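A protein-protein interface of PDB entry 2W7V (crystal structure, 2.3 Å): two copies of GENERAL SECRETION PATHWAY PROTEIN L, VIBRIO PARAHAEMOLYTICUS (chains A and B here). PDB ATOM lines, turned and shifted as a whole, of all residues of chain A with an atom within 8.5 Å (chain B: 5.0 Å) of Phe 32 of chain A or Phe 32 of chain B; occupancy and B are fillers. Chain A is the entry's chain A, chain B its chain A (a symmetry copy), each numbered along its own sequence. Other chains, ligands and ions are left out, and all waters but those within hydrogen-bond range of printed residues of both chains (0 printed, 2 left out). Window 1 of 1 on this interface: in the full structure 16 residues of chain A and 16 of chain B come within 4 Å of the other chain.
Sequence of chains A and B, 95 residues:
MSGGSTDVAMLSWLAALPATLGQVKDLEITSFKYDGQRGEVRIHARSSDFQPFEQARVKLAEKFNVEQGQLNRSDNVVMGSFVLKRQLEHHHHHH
O of Phe 32 of chain A is in hydrogen-bond range of N of Tyr 34 of chain B (2.8 Å). N of Tyr 34 of chain A sits at hydrogen-bond distance from O of Phe 32 of chain B (2.8 Å). N of Gly 36 of chain A sits at hydrogen-bond distance from O of Thr 30 of chain B (2.8 Å).
N of Lys 33 of chain A is in hydrogen-bond range of O of Arg 42 of chain A (2.7 Å). The backbone carbonyl oxygen of Glu 40 of chain A is in hydrogen-bond range of the backbone NH of Asp 35 of chain A (2.9 Å). NH1 of Arg 42 of chain A lies within salt-bridge range of OD2 of Asp 35 of chain A, 3.9 Å away. N of Thr 30 of chain B lies within hydrogen-bond range of O of His 44 of chain B. The backbone carbonyl oxygen (O) of Ser 31 of chain B sits at hydrogen-bond distance from the backbone NH (N) of His 44 of chain B (2.9 Å). O of Arg 42 of chain B sits at hydrogen-bond distance from N of Lys 33 of chain B.
Leu 11 of chain A touches Phe 32 of chain B. Leu 14 of chain A touches Phe 32 of chain B (CD1 to CZ, 3.1 Å). Leu 11 of chain B touches Pro 18 of chain A (O to CB, 3.4 Å). Ile 29 of chain A touches Leu 11 of chain B (CB to CD2, 3.95 Å). Ile 29 of chain A touches Tyr 34 of chain B. O of Tyr 34 of chain B touches CA of Ser 31 of chain A (3.1 Å). Phe 32 of chain A touches Leu 14 of chain B (CZ to CD1, 3.1 Å). CA of Lys 33 of chain A touches O of Phe 32 of chain B, at 3.4 Å. Tyr 34 of chain A touches Ser 31 of chain B (O to CA, 3.1 Å). Asp 35 of chain A touches Thr 30 of chain B.
Of chain B, only Leu 11 (3.9 Å), Leu 14 (3.1 Å), Phe 32 (3.1 Å), Lys 33 (3.4 Å) and Tyr 34 (2.8 Å) come within 4 Å of Phe 32 of chain A. Phe 32 of chain B touches just these residues of chain A: Leu 11, Leu 14, Phe 32, Lys 33 and Tyr 34. Of the printed residues of chain B, Ser 31 of chain A touches Tyr 34. Printed residues of chain B within 4 Å of Lys 33 of chain A: Phe 32 (3.4 Å). Of the printed residues of chain B, Gly 36 of chain A touches Thr 30. Printed residues of chain B within 4 Å of Ile 29 of chain A: Leu 11 and Tyr 34. Of the printed residues of chain A, Thr 30 of chain B touches Asp 35 (3.7 Å) and Gly 36 (2.8 Å). Ser 12 of chain A touches none of the printed residues of chain B. Arg 42 of chain A touches none of the printed residues of chain B. The nearest residue of chain A that does not touch Phe 32 of chain B is Asp 35 of chain A (5.1 Å). The nearest printed residue of chain A that does not touch Leu 14 of chain B is Leu 14 of chain A (4.8 Å).
Of the 24 printed residues of chain A, 10 touch a printed residue of chain B. Printed residues of chain B that touch a printed residue of chain A: Leu 11, Leu 14, Ile 29, Thr 30, Ser 31, Phe 32, Lys 33 and Tyr 34. Among the printed residues, 19 pairs touch across the chains.
Leu 11 of chain A touches Ile 29 of chain B, and with the chains exchanged Ile 29 of chain A touches Leu 11 of chain B. Leu 14 of chain A touches Phe 32 of chain B, and with the chains exchanged Phe 32 of chain A touches Leu 14 of chain B. Ile 29 of chain A touches Tyr 34 of chain B, and with the chains exchanged Tyr 34 of chain A touches Ile 29 of chain B. Phe 32 of chain A touches Lys 33 of chain B, and with the chains exchanged Lys 33 of chain A touches Phe 32 of chain B. 12 positions are printed for both chains. Of the 19 pairs that touch across the chains among the printed residues, 15 have their exchanged pair printed and touching as well.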
ATOM      1  N   MET A  10      24.518 -12.883  -0.686  1.00  0.00           N
ATOM      2  CA  MET A  10      23.292 -12.105  -0.625  1.00  0.00           C
ATOM      3  C   MET A  10      23.466 -10.729   0.059  1.00  0.00           C
ATOM      4  O   MET A  10      22.906  -9.748  -0.387  1.00  0.00           O
ATOM      5  CB  MET A  10      22.195 -12.915   0.060  1.00  0.00           C
ATOM      6  CG  MET A  10      20.850 -12.200   0.047  1.00  0.00           C
ATOM      7  SD  MET A  10      19.977 -11.939  -1.706  1.00  0.00           S
ATOM      8  CE  MET A  10      19.686 -13.786  -2.123  1.00  0.00           C
ATOM      9  N   LEU A  11      24.240 -10.671   1.128  1.00  0.00           N
ATOM     10  CA  LEU A  11      24.545  -9.401   1.767  1.00  0.00           C
ATOM     11  C   LEU A  11      25.192  -8.423   0.783  1.00  0.00           C
ATOM     12  O   LEU A  11      24.821  -7.271   0.709  1.00  0.00           O
ATOM     13  CB  LEU A  11      25.441  -9.624   2.992  1.00  0.00           C
ATOM     14  CG  LEU A  11      25.640  -8.456   3.954  1.00  0.00           C
ATOM     15  CD1 LEU A  11      24.315  -7.978   4.479  1.00  0.00           C
ATOM     16  CD2 LEU A  11      26.521  -8.910   5.091  1.00  0.00           C
ATOM     17  N   SER A  12      26.136  -8.901  -0.008  1.00  0.00           N
ATOM     18  CA  SER A  12      26.767  -8.059  -1.006  1.00  0.00           C
ATOM     19  C   SER A  12      25.799  -7.554  -2.072  1.00  0.00           C
ATOM     20  O   SER A  12      25.774  -6.337  -2.339  1.00  0.00           O
ATOM     21  CB  SER A  12      27.940  -8.792  -1.651  1.00  0.00           C
ATOM     22  OG  SER A  12      28.908  -9.139  -0.662  1.00  0.00           O
ATOM     23  N   LEU A  14      22.467  -7.526  -2.158  1.00  0.00           N
ATOM     24  CA  LEU A  14      21.450  -6.671  -1.595  1.00  0.00           C
ATOM     25  C   LEU A  14      21.700  -5.141  -1.832  1.00  0.00           C
ATOM     26  O   LEU A  14      20.768  -4.337  -1.883  1.00  0.00           O
ATOM     27  CB  LEU A  14      21.400  -7.026  -0.100  1.00  0.00           C
ATOM     28  CG  LEU A  14      20.767  -6.124   0.930  1.00  0.00           C
ATOM     29  CD1 LEU A  14      20.346  -6.982   2.126  1.00  0.00           C
ATOM     30  CD2 LEU A  14      21.751  -5.045   1.285  1.00  0.00           C
ATOM     31  N   ALA A  15      22.966  -4.746  -1.937  1.00  0.00           N
ATOM     32  CA  ALA A  15      23.365  -3.346  -2.226  1.00  0.00           C
ATOM     33  C   ALA A  15      22.801  -2.781  -3.570  1.00  0.00           C
ATOM     34  O   ALA A  15      22.680  -1.559  -3.739  1.00  0.00           O
ATOM     35  CB  ALA A  15      24.881  -3.247  -2.215  1.00  0.00           C
ATOM     36  N   LEU A  17      19.711  -3.544  -4.692  1.00  0.00           N
ATOM     37  CA  LEU A  17      18.264  -3.566  -4.651  1.00  0.00           C
ATOM     38  C   LEU A  17      17.602  -2.178  -4.576  1.00  0.00           C
ATOM     39  O   LEU A  17      16.589  -1.944  -5.241  1.00  0.00           O
ATOM     40  CB  LEU A  17      17.774  -4.484  -3.521  1.00  0.00           C
ATOM     41  CG  LEU A  17      17.915  -6.002  -3.760  1.00  0.00           C
ATOM     42  CD1 LEU A  17      17.518  -6.784  -2.500  1.00  0.00           C
ATOM     43  CD2 LEU A  17      17.095  -6.487  -4.974  1.00  0.00           C
ATOM     44  N   PRO A  18      18.162  -1.251  -3.775  1.00  0.00           N
ATOM     45  CA  PRO A  18      17.577   0.077  -3.804  1.00  0.00           C
ATOM     46  C   PRO A  18      17.614   0.709  -5.179  1.00  0.00           C
ATOM     47  O   PRO A  18      16.592   1.242  -5.634  1.00  0.00           O
ATOM     48  CB  PRO A  18      18.436   0.852  -2.788  1.00  0.00           C
ATOM     49  CG  PRO A  18      18.859  -0.223  -1.786  1.00  0.00           C
ATOM     50  CD  PRO A  18      19.259  -1.308  -2.780  1.00  0.00           C
ATOM     51  N   LEU A  21      15.041  -1.336  -7.471  1.00  0.00           N
ATOM     52  CA  LEU A  21      13.634  -1.052  -7.175  1.00  0.00           C
ATOM     53  C   LEU A  21      13.344   0.397  -7.499  1.00  0.00           C
ATOM     54  O   LEU A  21      12.247   0.754  -7.853  1.00  0.00           O
ATOM     55  CB  LEU A  21      13.271  -1.364  -5.710  1.00  0.00           C
ATOM     56  CG  LEU A  21      13.476  -2.805  -5.219  1.00  0.00           C
ATOM     57  CD1 LEU A  21      13.566  -2.840  -3.695  1.00  0.00           C
ATOM     58  CD2 LEU A  21      12.423  -3.747  -5.728  1.00  0.00           C
ATOM     59  N   ILE A  29       8.904   1.115  -1.465  1.00  0.00           N
ATOM     60  CA  ILE A  29       9.368   0.103  -0.501  1.00  0.00           C
ATOM     61  C   ILE A  29       9.081   0.539   0.921  1.00  0.00           C
ATOM     62  O   ILE A  29       9.666   1.476   1.407  1.00  0.00           O
ATOM     63  CB  ILE A  29      10.880  -0.204  -0.660  1.00  0.00           C
ATOM     64  CG1 ILE A  29      11.192  -0.475  -2.129  1.00  0.00           C
ATOM     65  CG2 ILE A  29      11.325  -1.425   0.224  1.00  0.00           C
ATOM     66  CD1 ILE A  29      10.285  -1.484  -2.818  1.00  0.00           C
ATOM     67  N   THR A  30       8.150  -0.139   1.579  1.00  0.00           N
ATOM     68  CA  THR A  30       7.805   0.167   2.952  1.00  0.00           C
ATOM     69  C   THR A  30       8.704  -0.584   3.965  1.00  0.00           C
ATOM     70  O   THR A  30       8.992  -0.083   5.062  1.00  0.00           O
ATOM     71  CB  THR A  30       6.339  -0.144   3.205  1.00  0.00           C
ATOM     72  OG1 THR A  30       6.096  -1.503   2.914  1.00  0.00           O
ATOM     73  CG2 THR A  30       5.443   0.706   2.321  1.00  0.00           C
ATOM     74  N   SER A  31       9.178  -1.776   3.603  1.00  0.00           N
ATOM     75  CA  SER A  31      10.196  -2.415   4.432  1.00  0.00           C
ATOM     76  C   SER A  31      10.960  -3.464   3.697  1.00  0.00           C
ATOM     77  O   SER A  31      10.520  -3.972   2.710  1.00  0.00           O
ATOM     78  CB  SER A  31       9.574  -3.070   5.669  1.00  0.00           C
ATOM     79  OG  SER A  31       9.077  -4.347   5.349  1.00  0.00           O
ATOM     80  N   PHE A  32      12.127  -3.794   4.210  1.00  0.00           N
ATOM     81  CA  PHE A  32      12.793  -4.977   3.751  1.00  0.00           C
ATOM     82  C   PHE A  32      13.743  -5.558   4.749  1.00  0.00           C
ATOM     83  O   PHE A  32      14.418  -4.827   5.477  1.00  0.00           O
ATOM     84  CB  PHE A  32      13.445  -4.747   2.406  1.00  0.00           C
ATOM     85  CG  PHE A  32      14.787  -4.164   2.464  1.00  0.00           C
ATOM     86  CD1 PHE A  32      15.001  -2.908   2.005  1.00  0.00           C
ATOM     87  CD2 PHE A  32      15.850  -4.929   2.883  1.00  0.00           C
ATOM     88  CE1 PHE A  32      16.279  -2.346   2.046  1.00  0.00           C
ATOM     89  CE2 PHE A  32      17.092  -4.439   2.932  1.00  0.00           C
ATOM     90  CZ  PHE A  32      17.343  -3.116   2.528  1.00  0.00           C
ATOM     91  N   LYS A  33      13.801  -6.887   4.752  1.00  0.00           N
ATOM     92  CA  LYS A  33      14.601  -7.609   5.716  1.00  0.00           C
ATOM     93  C   LYS A  33      15.522  -8.585   5.077  1.00  0.00           C
ATOM     94  O   LYS A  33      15.071  -9.420   4.348  1.00  0.00           O
ATOM     95  CB  LYS A  33      13.701  -8.389   6.669  1.00  0.00           C
ATOM     96  CG  LYS A  33      14.493  -9.094   7.783  1.00  0.00           C
ATOM     97  CD  LYS A  33      13.709  -9.297   9.009  1.00  0.00           C
ATOM     98  CE  LYS A  33      14.600  -9.632  10.208  1.00  0.00           C
ATOM     99  NZ  LYS A  33      13.815  -9.327  11.505  1.00  0.00           N
ATOM    100  N   TYR A  34      16.803  -8.492   5.395  1.00  0.00           N
ATOM    101  CA  TYR A  34      17.807  -9.533   5.168  1.00  0.00           C
ATOM    102  C   TYR A  34      17.945 -10.459   6.374  1.00  0.00           C
ATOM    103  O   TYR A  34      18.099  -9.985   7.533  1.00  0.00           O
ATOM    104  CB  TYR A  34      19.164  -8.898   4.882  1.00  0.00           C
ATOM    105  CG  TYR A  34      20.345  -9.837   4.868  1.00  0.00           C
ATOM    106  CD1 TYR A  34      20.620 -10.658   3.769  1.00  0.00           C
ATOM    107  CD2 TYR A  34      21.227  -9.881   5.948  1.00  0.00           C
ATOM    108  CE1 TYR A  34      21.742 -11.517   3.773  1.00  0.00           C
ATOM    109  CE2 TYR A  34      22.298 -10.708   5.962  1.00  0.00           C
ATOM    110  CZ  TYR A  34      22.565 -11.527   4.890  1.00  0.00           C
ATOM    111  OH  TYR A  34      23.678 -12.338   4.996  1.00  0.00           O
ATOM    112  N   ASP A  35      17.916 -11.764   6.081  1.00  0.00           N
ATOM    113  CA  ASP A  35      18.112 -12.836   7.060  1.00  0.00           C
ATOM    114  C   ASP A  35      19.345 -13.624   6.577  1.00  0.00           C
ATOM    115  O   ASP A  35      19.288 -14.369   5.598  1.00  0.00           O
ATOM    116  CB  ASP A  35      16.833 -13.695   7.129  1.00  0.00           C
ATOM    117  CG  ASP A  35      16.975 -14.944   7.958  1.00  0.00           C
ATOM    118  OD1 ASP A  35      17.990 -15.179   8.638  1.00  0.00           O
ATOM    119  OD2 ASP A  35      16.007 -15.716   7.941  1.00  0.00           O
ATOM    120  N   GLY A  36      20.467 -13.428   7.250  1.00  0.00           N
ATOM    121  CA  GLY A  36      21.723 -14.021   6.824  1.00  0.00           C
ATOM    122  C   GLY A  36      21.764 -15.521   6.968  1.00  0.00           C
ATOM    123  O   GLY A  36      22.469 -16.207   6.222  1.00  0.00           O
ATOM    124  N   GLU A  40      18.095 -14.838   2.657  1.00  0.00           N
ATOM    125  CA  GLU A  40      16.961 -14.293   1.954  1.00  0.00           C
ATOM    126  C   GLU A  40      16.832 -12.848   2.262  1.00  0.00           C
ATOM    127  O   GLU A  40      17.215 -12.392   3.328  1.00  0.00           O
ATOM    128  CB  GLU A  40      15.659 -14.907   2.424  1.00  0.00           C
ATOM    129  CG  GLU A  40      15.551 -16.365   2.318  1.00  0.00           C
ATOM    130  CD  GLU A  40      14.212 -16.862   2.842  1.00  0.00           C
ATOM    131  OE1 GLU A  40      13.444 -16.052   3.420  1.00  0.00           O
ATOM    132  OE2 GLU A  40      13.951 -18.048   2.690  1.00  0.00           O
ATOM    133  N   VAL A  41      16.200 -12.156   1.340  1.00  0.00           N
ATOM    134  CA  VAL A  41      15.681 -10.850   1.540  1.00  0.00           C
ATOM    135  C   VAL A  41      14.153 -10.858   1.295  1.00  0.00           C
ATOM    136  O   VAL A  41      13.675 -11.341   0.286  1.00  0.00           O
ATOM    137  CB  VAL A  41      16.391  -9.868   0.580  1.00  0.00           C
ATOM    138  CG1 VAL A  41      15.901  -8.424   0.788  1.00  0.00           C
ATOM    139  CG2 VAL A  41      17.950  -9.931   0.794  1.00  0.00           C
ATOM    140  N   ARG A  42      13.396 -10.314   2.240  1.00  0.00           N
ATOM    141  CA  ARG A  42      11.976 -10.105   2.048  1.00  0.00           C
ATOM    142  C   ARG A  42      11.640  -8.609   2.008  1.00  0.00           C
ATOM    143  O   ARG A  42      12.040  -7.837   2.866  1.00  0.00           O
ATOM    144  CB  ARG A  42      11.225 -10.831   3.140  1.00  0.00           C
ATOM    145  CG  ARG A  42      11.735 -12.266   3.330  1.00  0.00           C
ATOM    146  CD  ARG A  42      10.986 -12.982   4.449  1.00  0.00           C
ATOM    147  NE  ARG A  42      11.501 -12.617   5.772  1.00  0.00           N
ATOM    148  CZ  ARG A  42      12.636 -13.073   6.284  1.00  0.00           C
ATOM    149  NH1 ARG A  42      13.416 -13.900   5.596  1.00  0.00           N
ATOM    150  NH2 ARG A  42      12.998 -12.688   7.491  1.00  0.00           N
ATOM    151  N   ILE A  43      10.895  -8.226   0.989  1.00  0.00           N
ATOM    152  CA  ILE A  43      10.573  -6.860   0.676  1.00  0.00           C
ATOM    153  C   ILE A  43       9.075  -6.633   0.675  1.00  0.00           C
ATOM    154  O   ILE A  43       8.379  -7.327  -0.009  1.00  0.00           O
ATOM    155  CB  ILE A  43      11.067  -6.548  -0.763  1.00  0.00           C
ATOM    156  CG1 ILE A  43      12.616  -6.687  -0.861  1.00  0.00           C
ATOM    157  CG2 ILE A  43      10.673  -5.137  -1.153  1.00  0.00           C
ATOM    158  CD1 ILE A  43      13.151  -6.827  -2.296  1.00  0.00           C
ATOM    159  N   HIS A  44       8.574  -5.655   1.414  1.00  0.00           N
ATOM    160  CA  HIS A  44       7.212  -5.231   1.228  1.00  0.00           C
ATOM    161  C   HIS A  44       7.227  -3.917   0.471  1.00  0.00           C
ATOM    162  O   HIS A  44       8.106  -3.113   0.671  1.00  0.00           O
ATOM    163  CB  HIS A  44       6.444  -5.083   2.542  1.00  0.00           C
ATOM    164  CG  HIS A  44       6.408  -6.328   3.371  1.00  0.00           C
ATOM    165  ND1 HIS A  44       5.987  -6.333   4.690  1.00  0.00           N
ATOM    166  CD2 HIS A  44       6.779  -7.601   3.094  1.00  0.00           C
ATOM    167  CE1 HIS A  44       6.091  -7.562   5.174  1.00  0.00           C
ATOM    168  NE2 HIS A  44       6.562  -8.349   4.221  1.00  0.00           N
ATOM    169  N   ALA A  45       6.265  -3.740  -0.439  1.00  0.00           N
ATOM    170  CA  ALA A  45       6.101  -2.517  -1.229  1.00  0.00           C
ATOM    171  C   ALA A  45       4.621  -2.232  -1.499  1.00  0.00           C
ATOM    172  O   ALA A  45       3.742  -3.060  -1.268  1.00  0.00           O
ATOM    173  CB  ALA A  45       6.906  -2.623  -2.555  1.00  0.00           C
ATOM    174  N   PHE A  82       7.834  -9.574  -1.859  1.00  0.00           N
ATOM    175  CA  PHE A  82       8.750 -10.397  -2.613  1.00  0.00           C
ATOM    176  C   PHE A  82       9.677 -11.067  -1.626  1.00  0.00           C
ATOM    177  O   PHE A  82      10.073 -10.459  -0.644  1.00  0.00           O
ATOM    178  CB  PHE A  82       9.621  -9.519  -3.503  1.00  0.00           C
ATOM    179  CG  PHE A  82       8.893  -8.855  -4.591  1.00  0.00           C
ATOM    180  CD1 PHE A  82       8.428  -9.577  -5.650  1.00  0.00           C
ATOM    181  CD2 PHE A  82       8.696  -7.480  -4.571  1.00  0.00           C
ATOM    182  CE1 PHE A  82       7.740  -8.968  -6.654  1.00  0.00           C
ATOM    183  CE2 PHE A  82       7.995  -6.851  -5.615  1.00  0.00           C
ATOM    184  CZ  PHE A  82       7.527  -7.597  -6.638  1.00  0.00           C
ATOM    185  N   LEU A  84      13.399 -12.867  -1.982  1.00  0.00           N
ATOM    186  CA  LEU A  84      14.556 -13.099  -2.835  1.00  0.00           C
ATOM    187  C   LEU A  84      15.484 -14.109  -2.175  1.00  0.00           C
ATOM    188  O   LEU A  84      15.760 -14.010  -0.981  1.00  0.00           O
ATOM    189  CB  LEU A  84      15.361 -11.800  -3.009  1.00  0.00           C
ATOM    190  CG  LEU A  84      14.627 -10.534  -3.408  1.00  0.00           C
ATOM    191  CD1 LEU A  84      15.628  -9.367  -3.621  1.00  0.00           C
ATOM    192  CD2 LEU A  84      13.784 -10.784  -4.629  1.00  0.00           C
ATOM    193  N   LEU B  11      16.712   4.590   2.301  1.00  0.00           N
ATOM    194  CA  LEU B  11      16.724   3.501   1.337  1.00  0.00           C
ATOM    195  C   LEU B  11      17.941   3.589   0.412  1.00  0.00           C
ATOM    196  O   LEU B  11      18.618   2.612   0.172  1.00  0.00           O
ATOM    197  CB  LEU B  11      15.418   3.490   0.531  1.00  0.00           C
ATOM    198  CG  LEU B  11      15.120   2.265  -0.329  1.00  0.00           C
ATOM    199  CD1 LEU B  11      15.107   1.022   0.517  1.00  0.00           C
ATOM    200  CD2 LEU B  11      13.781   2.457  -0.997  1.00  0.00           C
ATOM    201  N   LEU B  14      21.339   3.078   2.663  1.00  0.00           N
ATOM    202  CA  LEU B  14      21.427   1.691   3.052  1.00  0.00           C
ATOM    203  C   LEU B  14      22.328   0.820   2.110  1.00  0.00           C
ATOM    204  O   LEU B  14      22.907  -0.187   2.522  1.00  0.00           O
ATOM    205  CB  LEU B  14      19.975   1.187   3.095  1.00  0.00           C
ATOM    206  CG  LEU B  14      19.622  -0.280   3.075  1.00  0.00           C
ATOM    207  CD1 LEU B  14      18.245  -0.450   3.722  1.00  0.00           C
ATOM    208  CD2 LEU B  14      19.680  -0.762   1.654  1.00  0.00           C
ATOM    209  N   ILE B  29      27.052 -10.054  10.012  1.00  0.00           N
ATOM    210  CA  ILE B  29      25.660  -9.573   9.999  1.00  0.00           C
ATOM    211  C   ILE B  29      24.689 -10.729   9.865  1.00  0.00           C
ATOM    212  O   ILE B  29      24.629 -11.365   8.843  1.00  0.00           O
ATOM    213  CB  ILE B  29      25.409  -8.544   8.865  1.00  0.00           C
ATOM    214  CG1 ILE B  29      26.496  -7.473   8.902  1.00  0.00           C
ATOM    215  CG2 ILE B  29      23.990  -7.881   8.980  1.00  0.00           C
ATOM    216  CD1 ILE B  29      26.748  -6.839  10.262  1.00  0.00           C
ATOM    217  N   THR B  30      23.943 -11.009  10.925  1.00  0.00           N
ATOM    218  CA  THR B  30      22.962 -12.074  10.912  1.00  0.00           C
ATOM    219  C   THR B  30      21.584 -11.597  10.388  1.00  0.00           C
ATOM    220  O   THR B  30      20.834 -12.362   9.765  1.00  0.00           O
ATOM    221  CB  THR B  30      22.826 -12.679  12.299  1.00  0.00           C
ATOM    222  OG1 THR B  30      22.462 -11.668  13.213  1.00  0.00           O
ATOM    223  CG2 THR B  30      24.140 -13.291  12.756  1.00  0.00           C
ATOM    224  N   SER B  31      21.248 -10.327  10.610  1.00  0.00           N
ATOM    225  CA  SER B  31      20.064  -9.783   9.951  1.00  0.00           C
ATOM    226  C   SER B  31      20.071  -8.292   9.895  1.00  0.00           C
ATOM    227  O   SER B  31      20.747  -7.648  10.640  1.00  0.00           O
ATOM    228  CB  SER B  31      18.781 -10.217  10.665  1.00  0.00           C
ATOM    229  OG  SER B  31      18.521  -9.373  11.761  1.00  0.00           O
ATOM    230  N   PHE B  32      19.286  -7.744   8.992  1.00  0.00           N
ATOM    231  CA  PHE B  32      19.006  -6.339   9.055  1.00  0.00           C
ATOM    232  C   PHE B  32      17.716  -5.954   8.406  1.00  0.00           C
ATOM    233  O   PHE B  32      17.333  -6.518   7.378  1.00  0.00           O
ATOM    234  CB  PHE B  32      20.173  -5.529   8.536  1.00  0.00           C
ATOM    235  CG  PHE B  32      20.191  -5.335   7.085  1.00  0.00           C
ATOM    236  CD1 PHE B  32      21.157  -5.915   6.335  1.00  0.00           C
ATOM    237  CD2 PHE B  32      19.293  -4.475   6.497  1.00  0.00           C
ATOM    238  CE1 PHE B  32      21.190  -5.728   4.952  1.00  0.00           C
ATOM    239  CE2 PHE B  32      19.289  -4.257   5.179  1.00  0.00           C
ATOM    240  CZ  PHE B  32      20.235  -4.895   4.357  1.00  0.00           C
ATOM    241  N   LYS B  33      17.064  -4.964   9.011  1.00  0.00           N
ATOM    242  CA  LYS B  33      15.758  -4.531   8.564  1.00  0.00           C
ATOM    243  C   LYS B  33      15.693  -3.065   8.326  1.00  0.00           C
ATOM    244  O   LYS B  33      15.992  -2.318   9.212  1.00  0.00           O
ATOM    245  CB  LYS B  33      14.704  -4.869   9.613  1.00  0.00           C
ATOM    246  CG  LYS B  33      13.279  -4.526   9.149  1.00  0.00           C
ATOM    247  CD  LYS B  33      12.248  -5.361   9.781  1.00  0.00           C
ATOM    248  CE  LYS B  33      10.913  -5.281   9.038  1.00  0.00           C
ATOM    249  NZ  LYS B  33      10.066  -6.519   9.413  1.00  0.00           N
ATOM    250  N   TYR B  34      15.261  -2.673   7.139  1.00  0.00           N
ATOM    251  CA  TYR B  34      14.797  -1.324   6.814  1.00  0.00           C
ATOM    252  C   TYR B  34      13.290  -1.181   7.010  1.00  0.00           C
ATOM    253  O   TYR B  34      12.494  -2.021   6.508  1.00  0.00           O
ATOM    254  CB  TYR B  34      15.134  -0.989   5.363  1.00  0.00           C
ATOM    255  CG  TYR B  34      14.507   0.266   4.810  1.00  0.00           C
ATOM    256  CD1 TYR B  34      15.016   1.536   5.107  1.00  0.00           C
ATOM    257  CD2 TYR B  34      13.415   0.190   3.946  1.00  0.00           C
ATOM    258  CE1 TYR B  34      14.420   2.696   4.562  1.00  0.00           C
ATOM    259  CE2 TYR B  34      12.835   1.298   3.428  1.00  0.00           C
ATOM    260  CZ  TYR B  34      13.322   2.549   3.727  1.00  0.00           C
ATOM    261  OH  TYR B  34      12.664   3.620   3.155  1.00  0.00           O
ATOM    262  N   VAL B  41      17.089   1.691   9.939  1.00  0.00           N
ATOM    263  CA  VAL B  41      17.627   0.397   9.719  1.00  0.00           C
ATOM    264  C   VAL B  41      18.077  -0.213  11.069  1.00  0.00           C
ATOM    265  O   VAL B  41      18.790   0.405  11.837  1.00  0.00           O
ATOM    266  CB  VAL B  41      18.815   0.500   8.735  1.00  0.00           C
ATOM    267  CG1 VAL B  41      19.409  -0.885   8.421  1.00  0.00           C
ATOM    268  CG2 VAL B  41      18.353   1.191   7.397  1.00  0.00           C
ATOM    269  N   ARG B  42      17.644  -1.437  11.343  1.00  0.00           N
ATOM    270  CA  ARG B  42      18.136  -2.178  12.487  1.00  0.00           C
ATOM    271  C   ARG B  42      18.943  -3.404  12.044  1.00  0.00           C
ATOM    272  O   ARG B  42      18.512  -4.194  11.218  1.00  0.00           O
ATOM    273  CB  ARG B  42      16.964  -2.551  13.364  1.00  0.00           C
ATOM    274  CG  ARG B  42      16.028  -1.359  13.610  1.00  0.00           C
ATOM    275  CD  ARG B  42      14.838  -1.753  14.478  1.00  0.00           C
ATOM    276  NE  ARG B  42      13.791  -2.422  13.700  1.00  0.00           N
ATOM    277  CZ  ARG B  42      12.951  -1.797  12.886  1.00  0.00           C
ATOM    278  NH1 ARG B  42      13.022  -0.483  12.702  1.00  0.00           N
ATOM    279  NH2 ARG B  42      12.038  -2.497  12.243  1.00  0.00           N
ATOM    280  N   ILE B  43      20.124  -3.537  12.616  1.00  0.00           N
ATOM    281  CA  ILE B  43      21.102  -4.527  12.257  1.00  0.00           C
ATOM    282  C   ILE B  43      21.450  -5.413  13.435  1.00  0.00           C
ATOM    283  O   ILE B  43      21.816  -4.907  14.458  1.00  0.00           O
ATOM    284  CB  ILE B  43      22.415  -3.807  11.845  1.00  0.00           C
ATOM    285  CG1 ILE B  43      22.187  -2.911  10.590  1.00  0.00           C
ATOM    286  CG2 ILE B  43      23.493  -4.826  11.534  1.00  0.00           C
ATOM    287  CD1 ILE B  43      23.272  -1.845  10.365  1.00  0.00           C
ATOM    288  N   HIS B  44      21.363  -6.726  13.299  1.00  0.00           N
ATOM    289  CA  HIS B  44      21.943  -7.598  14.286  1.00  0.00           C
ATOM    290  C   HIS B  44      23.226  -8.170  13.714  1.00  0.00           C
ATOM    291  O   HIS B  44      23.301  -8.428  12.535  1.00  0.00           O
ATOM    292  CB  HIS B  44      21.004  -8.723  14.721  1.00  0.00           C
ATOM    293  CG  HIS B  44      19.695  -8.247  15.270  1.00  0.00           C
ATOM    294  ND1 HIS B  44      18.623  -9.096  15.481  1.00  0.00           N
ATOM    295  CD2 HIS B  44      19.263  -7.009  15.610  1.00  0.00           C
ATOM    296  CE1 HIS B  44      17.598  -8.394  15.941  1.00  0.00           C
ATOM    297  NE2 HIS B  44      17.965  -7.127  16.035  1.00  0.00           N
